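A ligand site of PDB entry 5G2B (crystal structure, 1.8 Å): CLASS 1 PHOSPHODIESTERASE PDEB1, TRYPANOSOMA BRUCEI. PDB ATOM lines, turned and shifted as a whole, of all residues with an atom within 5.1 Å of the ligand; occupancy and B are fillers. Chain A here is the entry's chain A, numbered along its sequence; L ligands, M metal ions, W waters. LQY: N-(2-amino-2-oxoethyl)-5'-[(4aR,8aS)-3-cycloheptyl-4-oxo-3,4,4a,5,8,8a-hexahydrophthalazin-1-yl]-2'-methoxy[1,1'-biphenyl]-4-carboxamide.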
ATOM      1  N   TYR A 110      33.505 -12.713   0.379  1.00  0.00           N
ATOM      2  CA  TYR A 110      33.902 -11.481  -0.284  1.00  0.00           C
ATOM      3  C   TYR A 110      34.665 -10.493   0.624  1.00  0.00           C
ATOM      4  O   TYR A 110      35.799 -10.140   0.298  1.00  0.00           O
ATOM      5  CB  TYR A 110      32.725 -10.793  -0.983  1.00  0.00           C
ATOM      6  CG  TYR A 110      33.161  -9.589  -1.789  1.00  0.00           C
ATOM      7  CD1 TYR A 110      33.668  -9.737  -3.073  1.00  0.00           C
ATOM      8  CD2 TYR A 110      33.063  -8.304  -1.272  1.00  0.00           C
ATOM      9  CE1 TYR A 110      34.057  -8.643  -3.831  1.00  0.00           C
ATOM     10  CE2 TYR A 110      33.446  -7.187  -2.023  1.00  0.00           C
ATOM     11  CZ  TYR A 110      33.946  -7.375  -3.296  1.00  0.00           C
ATOM     12  OH  TYR A 110      34.336  -6.301  -4.018  1.00  0.00           O
ATOM     13  N   HIS A 111      34.086 -10.034   1.755  1.00  0.00           N
ATOM     14  CA  HIS A 111      34.762  -9.013   2.582  1.00  0.00           C
ATOM     15  C   HIS A 111      35.722  -9.637   3.567  1.00  0.00           C
ATOM     16  O   HIS A 111      35.636  -9.468   4.784  1.00  0.00           O
ATOM     17  CB  HIS A 111      33.774  -8.094   3.313  1.00  0.00           C
ATOM     18  CG  HIS A 111      32.938  -7.255   2.402  1.00  0.00           C
ATOM     19  ND1 HIS A 111      31.643  -7.569   2.100  1.00  0.00           N
ATOM     20  CD2 HIS A 111      33.206  -6.107   1.746  1.00  0.00           C
ATOM     21  CE1 HIS A 111      31.138  -6.649   1.292  1.00  0.00           C
ATOM     22  NE2 HIS A 111      32.075  -5.750   1.054  1.00  0.00           N
ATOM     23  N   THR A 225      32.922   5.118   2.102  1.00  0.00           N
ATOM     24  CA  THR A 225      32.654   3.903   1.373  1.00  0.00           C
ATOM     25  C   THR A 225      31.253   3.361   1.621  1.00  0.00           C
ATOM     26  O   THR A 225      30.893   2.361   0.951  1.00  0.00           O
ATOM     27  CB  THR A 225      33.624   2.754   1.740  1.00  0.00           C
ATOM     28  OG1 THR A 225      33.556   2.473   3.136  1.00  0.00           O
ATOM     29  CG2 THR A 225      34.999   3.169   1.407  1.00  0.00           C
ATOM     30  N   MET A 227      27.884   2.807   0.716  1.00  0.00           N
ATOM     31  CA  MET A 227      27.205   3.019  -0.584  1.00  0.00           C
ATOM     32  C   MET A 227      25.911   3.800  -0.486  1.00  0.00           C
ATOM     33  O   MET A 227      25.418   4.307  -1.498  1.00  0.00           O
ATOM     34  CB  MET A 227      27.016   1.690  -1.380  1.00  0.00           C
ATOM     35  CG  MET A 227      28.308   1.146  -1.971  1.00  0.00           C
ATOM     36  SD  MET A 227      29.107   2.300  -3.136  1.00  0.00           S
ATOM     37  CE  MET A 227      28.184   1.893  -4.608  1.00  0.00           C
ATOM     38  N   ASP A 264      36.903   0.266  -4.303  1.00  0.00           N
ATOM     39  CA  ASP A 264      35.894  -0.616  -3.738  1.00  0.00           C
ATOM     40  C   ASP A 264      34.884  -1.089  -4.764  1.00  0.00           C
ATOM     41  O   ASP A 264      34.303  -2.122  -4.578  1.00  0.00           O
ATOM     42  CB  ASP A 264      35.150   0.166  -2.635  1.00  0.00           C
ATOM     43  CG  ASP A 264      34.813  -0.640  -1.434  1.00  0.00           C
ATOM     44  OD1 ASP A 264      35.426  -1.709  -1.155  1.00  0.00           O
ATOM     45  OD2 ASP A 264      33.934  -0.085  -0.707  1.00  0.00           O
ATOM     46  N   ILE A 265      34.630  -0.341  -5.851  1.00  0.00           N
ATOM     47  CA  ILE A 265      33.779  -0.871  -6.913  1.00  0.00           C
ATOM     48  C   ILE A 265      34.546  -1.163  -8.193  1.00  0.00           C
ATOM     49  O   ILE A 265      33.968  -1.139  -9.269  1.00  0.00           O
ATOM     50  CB  ILE A 265      32.581   0.073  -7.259  1.00  0.00           C
ATOM     51  CG1 ILE A 265      33.047   1.471  -7.574  1.00  0.00           C
ATOM     52  CG2 ILE A 265      31.554   0.093  -6.121  1.00  0.00           C
ATOM     53  CD1 ILE A 265      31.926   2.363  -8.028  1.00  0.00           C
ATOM     54  N   ASN A 267      35.884  -3.973  -9.244  1.00  0.00           N
ATOM     55  CA  ASN A 267      35.864  -5.379  -9.704  1.00  0.00           C
ATOM     56  C   ASN A 267      35.559  -5.477 -11.182  1.00  0.00           C
ATOM     57  O   ASN A 267      36.137  -6.276 -11.878  1.00  0.00           O
ATOM     58  CB  ASN A 267      34.840  -6.231  -8.934  1.00  0.00           C
ATOM     59  CG  ASN A 267      35.210  -6.487  -7.470  1.00  0.00           C
ATOM     60  OD1 ASN A 267      34.341  -6.888  -6.707  1.00  0.00           O
ATOM     61  ND2 ASN A 267      36.437  -6.203  -7.057  1.00  0.00           N
ATOM     62  N   VAL A 268      34.654  -4.640 -11.663  1.00  0.00           N
ATOM     63  CA  VAL A 268      34.247  -4.669 -13.034  1.00  0.00           C
ATOM     64  C   VAL A 268      35.222  -3.957 -14.015  1.00  0.00           C
ATOM     65  O   VAL A 268      34.923  -3.904 -15.224  1.00  0.00           O
ATOM     66  CB  VAL A 268      32.858  -4.053 -13.236  1.00  0.00           C
ATOM     67  CG1 VAL A 268      31.766  -4.871 -12.522  1.00  0.00           C
ATOM     68  CG2 VAL A 268      32.853  -2.569 -12.847  1.00  0.00           C
ATOM     69  N   TRP A 278      35.374 -12.268  -8.777  1.00  0.00           N
ATOM     70  CA  TRP A 278      34.870 -11.347  -7.772  1.00  0.00           C
ATOM     71  C   TRP A 278      33.334 -11.463  -7.719  1.00  0.00           C
ATOM     72  O   TRP A 278      32.746 -11.520  -6.632  1.00  0.00           O
ATOM     73  CB  TRP A 278      35.312  -9.891  -8.026  1.00  0.00           C
ATOM     74  CG  TRP A 278      36.800  -9.620  -7.766  1.00  0.00           C
ATOM     75  CD1 TRP A 278      37.713  -9.136  -8.660  1.00  0.00           C
ATOM     76  CD2 TRP A 278      37.521  -9.832  -6.557  1.00  0.00           C
ATOM     77  NE1 TRP A 278      38.946  -9.020  -8.077  1.00  0.00           N
ATOM     78  CE2 TRP A 278      38.859  -9.420  -6.775  1.00  0.00           C
ATOM     79  CE3 TRP A 278      37.152 -10.291  -5.284  1.00  0.00           C
ATOM     80  CZ2 TRP A 278      39.825  -9.499  -5.786  1.00  0.00           C
ATOM     81  CZ3 TRP A 278      38.128 -10.348  -4.300  1.00  0.00           C
ATOM     82  CH2 TRP A 278      39.436  -9.953  -4.555  1.00  0.00           C
ATOM     83  N   ALA A 279      32.695 -11.406  -8.857  1.00  0.00           N
ATOM     84  CA  ALA A 279      31.246 -11.378  -8.902  1.00  0.00           C
ATOM     85  C   ALA A 279      30.633 -12.581  -8.225  1.00  0.00           C
ATOM     86  O   ALA A 279      29.610 -12.434  -7.562  1.00  0.00           O
ATOM     87  CB  ALA A 279      30.749 -11.293 -10.333  1.00  0.00           C
ATOM     88  N   VAL A 282      31.020 -12.086  -4.303  1.00  0.00           N
ATOM     89  CA  VAL A 282      30.018 -11.152  -3.719  1.00  0.00           C
ATOM     90  C   VAL A 282      28.631 -11.765  -3.738  1.00  0.00           C
ATOM     91  O   VAL A 282      27.888 -11.652  -2.766  1.00  0.00           O
ATOM     92  CB  VAL A 282      29.756  -9.767  -4.406  1.00  0.00           C
ATOM     93  CG1 VAL A 282      30.228  -8.596  -3.562  1.00  0.00           C
ATOM     94  CG2 VAL A 282      30.203  -9.665  -5.839  1.00  0.00           C
ATOM     95  N   THR A 283      28.300 -12.367  -4.878  1.00  0.00           N
ATOM     96  CA  THR A 283      27.002 -12.984  -5.092  1.00  0.00           C
ATOM     97  C   THR A 283      26.714 -13.988  -4.005  1.00  0.00           C
ATOM     98  O   THR A 283      25.620 -13.969  -3.403  1.00  0.00           O
ATOM     99  CB  THR A 283      26.868 -13.562  -6.502  1.00  0.00           C
ATOM    100  OG1 THR A 283      26.687 -12.479  -7.447  1.00  0.00           O
ATOM    101  CG2 THR A 283      25.650 -14.531  -6.564  1.00  0.00           C
ATOM    102  N   PHE A 286      26.144 -12.226  -0.653  1.00  0.00           N
ATOM    103  CA  PHE A 286      24.798 -11.665  -0.617  1.00  0.00           C
ATOM    104  C   PHE A 286      23.762 -12.771  -0.339  1.00  0.00           C
ATOM    105  O   PHE A 286      22.889 -12.623   0.545  1.00  0.00           O
ATOM    106  CB  PHE A 286      24.469 -10.896  -1.899  1.00  0.00           C
ATOM    107  CG  PHE A 286      25.084  -9.503  -1.977  1.00  0.00           C
ATOM    108  CD1 PHE A 286      26.000  -9.027  -1.054  1.00  0.00           C
ATOM    109  CD2 PHE A 286      24.729  -8.664  -3.023  1.00  0.00           C
ATOM    110  CE1 PHE A 286      26.542  -7.758  -1.180  1.00  0.00           C
ATOM    111  CE2 PHE A 286      25.248  -7.388  -3.147  1.00  0.00           C
ATOM    112  CZ  PHE A 286      26.171  -6.943  -2.228  1.00  0.00           C
ATOM    113  N   TYR A 287      23.902 -13.911  -1.026  1.00  0.00           N
ATOM    114  CA  TYR A 287      22.906 -14.957  -0.850  1.00  0.00           C
ATOM    115  C   TYR A 287      22.848 -15.476   0.566  1.00  0.00           C
ATOM    116  O   TYR A 287      21.758 -15.815   1.042  1.00  0.00           O
ATOM    117  CB  TYR A 287      23.074 -16.130  -1.820  1.00  0.00           C
ATOM    118  CG  TYR A 287      22.732 -15.847  -3.251  1.00  0.00           C
ATOM    119  CD1 TYR A 287      21.844 -14.827  -3.599  1.00  0.00           C
ATOM    120  CD2 TYR A 287      23.251 -16.656  -4.280  1.00  0.00           C
ATOM    121  CE1 TYR A 287      21.508 -14.588  -4.904  1.00  0.00           C
ATOM    122  CE2 TYR A 287      22.929 -16.409  -5.601  1.00  0.00           C
ATOM    123  CZ  TYR A 287      22.056 -15.371  -5.900  1.00  0.00           C
ATOM    124  OH  TYR A 287      21.688 -15.089  -7.186  1.00  0.00           O
ATOM    125  N   MET A 303      18.042  -9.303  -5.230  1.00  0.00           N
ATOM    126  CA  MET A 303      19.508  -9.429  -5.236  1.00  0.00           C
ATOM    127  C   MET A 303      20.131 -10.428  -4.240  1.00  0.00           C
ATOM    128  O   MET A 303      21.160 -11.040  -4.528  1.00  0.00           O
ATOM    129  CB  MET A 303      20.088  -8.019  -5.005  1.00  0.00           C
ATOM    130  CG  MET A 303      21.531  -7.879  -5.404  1.00  0.00           C
ATOM    131  SD  MET A 303      22.054  -6.151  -5.548  1.00  0.00           S
ATOM    132  CE  MET A 303      21.308  -5.682  -7.105  1.00  0.00           C
ATOM    133  N   ASN A 309      17.195 -15.964  -8.709  1.00  0.00           N
ATOM    134  CA  ASN A 309      18.134 -15.704  -9.822  1.00  0.00           C
ATOM    135  C   ASN A 309      18.816 -16.901 -10.351  1.00  0.00           C
ATOM    136  O   ASN A 309      19.313 -17.722  -9.596  1.00  0.00           O
ATOM    137  CB  ASN A 309      19.239 -14.736  -9.433  1.00  0.00           C
ATOM    138  CG  ASN A 309      19.231 -13.472 -10.273  1.00  0.00           C
ATOM    139  OD1 ASN A 309      19.224 -12.362  -9.723  1.00  0.00           O
ATOM    140  ND2 ASN A 309      19.270 -13.611 -11.602  1.00  0.00           N
ATOM    141  N   GLU A 311      21.214 -16.046 -13.051  1.00  0.00           N
ATOM    142  CA  GLU A 311      22.437 -15.561 -13.745  1.00  0.00           C
ATOM    143  C   GLU A 311      23.140 -14.225 -13.415  1.00  0.00           C
ATOM    144  O   GLU A 311      22.569 -13.114 -13.419  1.00  0.00           O
ATOM    145  CB  GLU A 311      22.261 -15.631 -15.273  1.00  0.00           C
ATOM    146  CG  GLU A 311      21.169 -14.736 -15.834  1.00  0.00           C
ATOM    147  CD  GLU A 311      20.894 -15.013 -17.323  1.00  0.00           C
ATOM    148  OE1 GLU A 311      21.830 -15.296 -18.099  1.00  0.00           O
ATOM    149  OE2 GLU A 311      19.716 -14.934 -17.724  1.00  0.00           O
ATOM    150  N   LEU A 312      24.436 -14.384 -13.197  1.00  0.00           N
ATOM    151  CA  LEU A 312      25.452 -13.318 -13.221  1.00  0.00           C
ATOM    152  C   LEU A 312      25.292 -12.278 -14.314  1.00  0.00           C
ATOM    153  O   LEU A 312      25.333 -11.086 -14.033  1.00  0.00           O
ATOM    154  CB  LEU A 312      26.826 -13.934 -13.379  1.00  0.00           C
ATOM    155  CG  LEU A 312      27.848 -14.018 -12.269  1.00  0.00           C
ATOM    156  CD1 LEU A 312      27.253 -14.159 -10.875  1.00  0.00           C
ATOM    157  CD2 LEU A 312      28.806 -15.161 -12.582  1.00  0.00           C
ATOM    158  N   GLY A 315      23.073  -9.396 -13.919  1.00  0.00           N
ATOM    159  CA  GLY A 315      23.419  -8.678 -12.721  1.00  0.00           C
ATOM    160  C   GLY A 315      24.674  -7.839 -12.891  1.00  0.00           C
ATOM    161  O   GLY A 315      24.698  -6.684 -12.483  1.00  0.00           O
ATOM    162  N   GLN A 316      25.693  -8.406 -13.535  1.00  0.00           N
ATOM    163  CA  GLN A 316      26.881  -7.641 -13.863  1.00  0.00           C
ATOM    164  C   GLN A 316      26.610  -6.491 -14.751  1.00  0.00           C
ATOM    165  O   GLN A 316      27.148  -5.409 -14.525  1.00  0.00           O
ATOM    166  CB  GLN A 316      28.009  -8.544 -14.387  1.00  0.00           C
ATOM    167  CG  GLN A 316      28.502  -9.485 -13.270  1.00  0.00           C
ATOM    168  CD  GLN A 316      29.040  -8.718 -12.060  1.00  0.00           C
ATOM    169  OE1 GLN A 316      30.161  -8.165 -12.083  1.00  0.00           O
ATOM    170  NE2 GLN A 316      28.247  -8.681 -10.999  1.00  0.00           N
ATOM    171  N   PHE A 319      24.800  -3.767 -12.804  1.00  0.00           N
ATOM    172  CA  PHE A 319      25.733  -3.063 -11.945  1.00  0.00           C
ATOM    173  C   PHE A 319      26.613  -2.118 -12.777  1.00  0.00           C
ATOM    174  O   PHE A 319      26.771  -0.911 -12.447  1.00  0.00           O
ATOM    175  CB  PHE A 319      26.552  -4.071 -11.120  1.00  0.00           C
ATOM    176  CG  PHE A 319      27.503  -3.426 -10.152  1.00  0.00           C
ATOM    177  CD1 PHE A 319      27.055  -2.943  -8.921  1.00  0.00           C
ATOM    178  CD2 PHE A 319      28.856  -3.267 -10.473  1.00  0.00           C
ATOM    179  CE1 PHE A 319      27.953  -2.369  -8.014  1.00  0.00           C
ATOM    180  CE2 PHE A 319      29.721  -2.669  -9.577  1.00  0.00           C
ATOM    181  CZ  PHE A 319      29.279  -2.210  -8.353  1.00  0.00           C
ATOM    182  N   VAL A 323      25.584   1.592 -11.710  1.00  0.00           N
ATOM    183  CA  VAL A 323      26.646   2.003 -10.807  1.00  0.00           C
ATOM    184  C   VAL A 323      28.042   2.319 -11.428  1.00  0.00           C
ATOM    185  O   VAL A 323      28.456   3.497 -11.434  1.00  0.00           O
ATOM    186  CB  VAL A 323      26.735   1.010  -9.663  1.00  0.00           C
ATOM    187  CG1 VAL A 323      27.676   1.540  -8.552  1.00  0.00           C
ATOM    188  CG2 VAL A 323      25.328   0.771  -9.096  1.00  0.00           C
HETATM  189  C   LQY L   1      31.034  -7.333  -8.675  1.00  0.00           C
HETATM  190  N   LQY L   1      23.091 -10.217  -7.737  1.00  0.00           N
HETATM  191  O   LQY L   1      29.686  -6.988  -8.346  1.00  0.00           O
HETATM  192  C1  LQY L   1      29.484  -6.203  -7.236  1.00  0.00           C
HETATM  193  N1  LQY L   1      22.232 -13.517  -8.939  1.00  0.00           N
HETATM  194  O1  LQY L   1      22.954  -8.847  -9.510  1.00  0.00           O
HETATM  195  C2  LQY L   1      30.484  -5.447  -6.621  1.00  0.00           C
HETATM  196  N2  LQY L   1      27.290  -3.531  -3.699  1.00  0.00           N
HETATM  197  O2  LQY L   1      23.588 -12.053  -9.976  1.00  0.00           O
HETATM  198  C3  LQY L   1      30.189  -4.721  -5.477  1.00  0.00           C
HETATM  199  N3  LQY L   1      26.915  -2.633  -2.706  1.00  0.00           N
HETATM  200  O3  LQY L   1      27.326  -1.582  -0.698  1.00  0.00           O
HETATM  201  C4  LQY L   1      28.893  -4.715  -4.937  1.00  0.00           C
HETATM  202  C5  LQY L   1      27.912  -5.490  -5.558  1.00  0.00           C
HETATM  203  C6  LQY L   1      28.183  -6.241  -6.698  1.00  0.00           C
HETATM  204  C7  LQY L   1      27.091  -7.107  -7.242  1.00  0.00           C
HETATM  205  C8  LQY L   1      26.543  -8.103  -6.453  1.00  0.00           C
HETATM  206  C9  LQY L   1      25.433  -8.825  -6.870  1.00  0.00           C
HETATM  207  C10 LQY L   1      24.841  -8.565  -8.099  1.00  0.00           C
HETATM  208  C11 LQY L   1      25.410  -7.587  -8.923  1.00  0.00           C
HETATM  209  C12 LQY L   1      26.519  -6.870  -8.490  1.00  0.00           C
HETATM  210  C13 LQY L   1      23.563  -9.235  -8.524  1.00  0.00           C
HETATM  211  C14 LQY L   1      22.168 -11.219  -8.232  1.00  0.00           C
HETATM  212  C15 LQY L   1      22.733 -12.308  -9.128  1.00  0.00           C
HETATM  213  C16 LQY L   1      28.534  -3.850  -3.790  1.00  0.00           C
HETATM  214  C17 LQY L   1      25.644  -2.019  -3.113  1.00  0.00           C
HETATM  215  C18 LQY L   1      25.856  -1.185  -4.458  1.00  0.00           C
HETATM  216  C19 LQY L   1      24.649  -0.669  -5.244  1.00  0.00           C
HETATM  217  C20 LQY L   1      23.628  -1.723  -5.649  1.00  0.00           C
HETATM  218  C21 LQY L   1      22.572  -2.065  -4.594  1.00  0.00           C
HETATM  219  C22 LQY L   1      23.016  -2.613  -3.220  1.00  0.00           C
HETATM  220  C23 LQY L   1      24.461  -3.118  -3.103  1.00  0.00           C
HETATM  221  C24 LQY L   1      27.629  -2.394  -1.547  1.00  0.00           C
HETATM  222  C25 LQY L   1      28.917  -3.191  -1.426  1.00  0.00           C
HETATM  223  C26 LQY L   1      29.945  -2.703  -0.394  1.00  0.00           C
HETATM  224  C27 LQY L   1      30.732  -1.531  -0.896  1.00  0.00           C
HETATM  225  C28 LQY L   1      30.844  -1.221  -2.191  1.00  0.00           C
HETATM  226  C29 LQY L   1      30.074  -1.926  -3.280  1.00  0.00           C
HETATM  227  C30 LQY L   1      29.570  -3.305  -2.818  1.00  0.00           C
HETATM  228 MG    MG M   1      32.885  -1.575   3.294  1.00  0.00          MG
HETATM  229 ZN    ZN M   2      35.361  -2.773   0.657  1.00  0.00          ZN
HETATM  230  O   HOH W   1      23.611 -11.927  -5.268  1.00  0.00           O
HETATM  231  O   HOH W   2      33.014  -7.849 -11.001  1.00  0.00           O
HETATM  232  O   HOH W   3      33.387  -3.571  -0.155  1.00  0.00           O
HETATM  233  O   HOH W   4      31.838  -3.042   2.442  1.00  0.00           O
HETATM  234  O   HOH W   5      28.385   0.050   1.237  1.00  0.00           O
HETATM  235  O   HOH W   6      22.748  -5.622 -10.298  1.00  0.00           O
HETATM  236  O   HOH W   7      25.855 -10.561 -10.896  1.00  0.00           O
HETATM  237  O   HOH W   8      33.004  -3.862  -2.731  1.00  0.00           O
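A nitrogen (N1) of the ligand lies within hydrogen-bond range of the side-chain hydroxyl (OH) of Tyr 287 (2.4 Å). The side-chain amide oxygen (OD1) of Asn 309 sits close to a nitrogen (N1) of the ligand (3.3 Å). The side-chain amide nitrogen of Gln 316 is in hydrogen-bond range of an oxygen (O) of the ligand (3.5 Å).
The side-chain amide nitrogen (ND2) of Asn 309 sits close to the backbone NH (N) of Glu 311 (3.4 Å). OD1 of Asn 267 lies within hydrogen-bond range of OH of Tyr 110 (2.8 Å). O of Ala 279 lies within hydrogen-bond range of OG1 of Thr 283 (2.9 Å).
His 111 touches the ligand. CG of Met 227 touches O3 of the ligand, at 3.2 Å. OD2 of Asp 264 touches C27 of the ligand, at 3.5 Å. Ile 265 touches the ligand (CG2 to C29, 3.8 Å). Asn 267 touches the ligand (OD1 to C, 3.9 Å). CG2 of Val 282 touches O of the ligand, 3.7 Å away. OG1 of Thr 283 touches C9 of the ligand, 3.9 Å away. Phe 286 touches the ligand (CE2 to C8, 3.6 Å). Met 303 touches the ligand. O of Glu 311 touches O2 of the ligand, at 3.7 Å. Leu 312 touches the ligand. CA of Gly 315 touches O1 of the ligand, 3.2 Å away. Phe 319 touches the ligand. Hydrophobic or aromatic side chains that line the ligand: Met 227, Ile 265, Val 282, Phe 286, Tyr 287, Met 303 and Phe 319. 16 residues have an atom within 4 Å of the ligand: His 111, Met 227, Asp 264, Ile 265, Asn 267, Val 282, Thr 283, Phe 286, Tyr 287, Met 303, Asn 309, Glu 311, Leu 312, Gly 315, Gln 316 and Phe 319. The nearest printed residue that does not touch the ligand is Ala 279 (4.1 Å).
Water W5 lies within hydrogen-bond range of an oxygen (O3) of the ligand (2.7 Å), the backbone NH of Met 227 (2.9 Å) and the backbone carbonyl oxygen of Thr 225 (3.4 Å). Water W7 lies within hydrogen-bond range of an oxygen (O2) of the ligand, the side-chain amide nitrogen (NE2) of Gln 316 and the backbone carbonyl oxygen (O) of Leu 312. Water W1 lies within hydrogen-bond range of O of Met 303 (2.7 Å), N of the ligand (3.0 Å) and O of Thr 283 (3.4 Å). Water W6 lies within hydrogen-bond range of O of Gly 315 (3.1 Å) and O1 of the ligand (3.3 Å). Water W8 bridges the backbone carbonyl oxygen of Asp 264 (2.9 Å) and the side-chain hydroxyl of Tyr 110 (3.1 Å).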
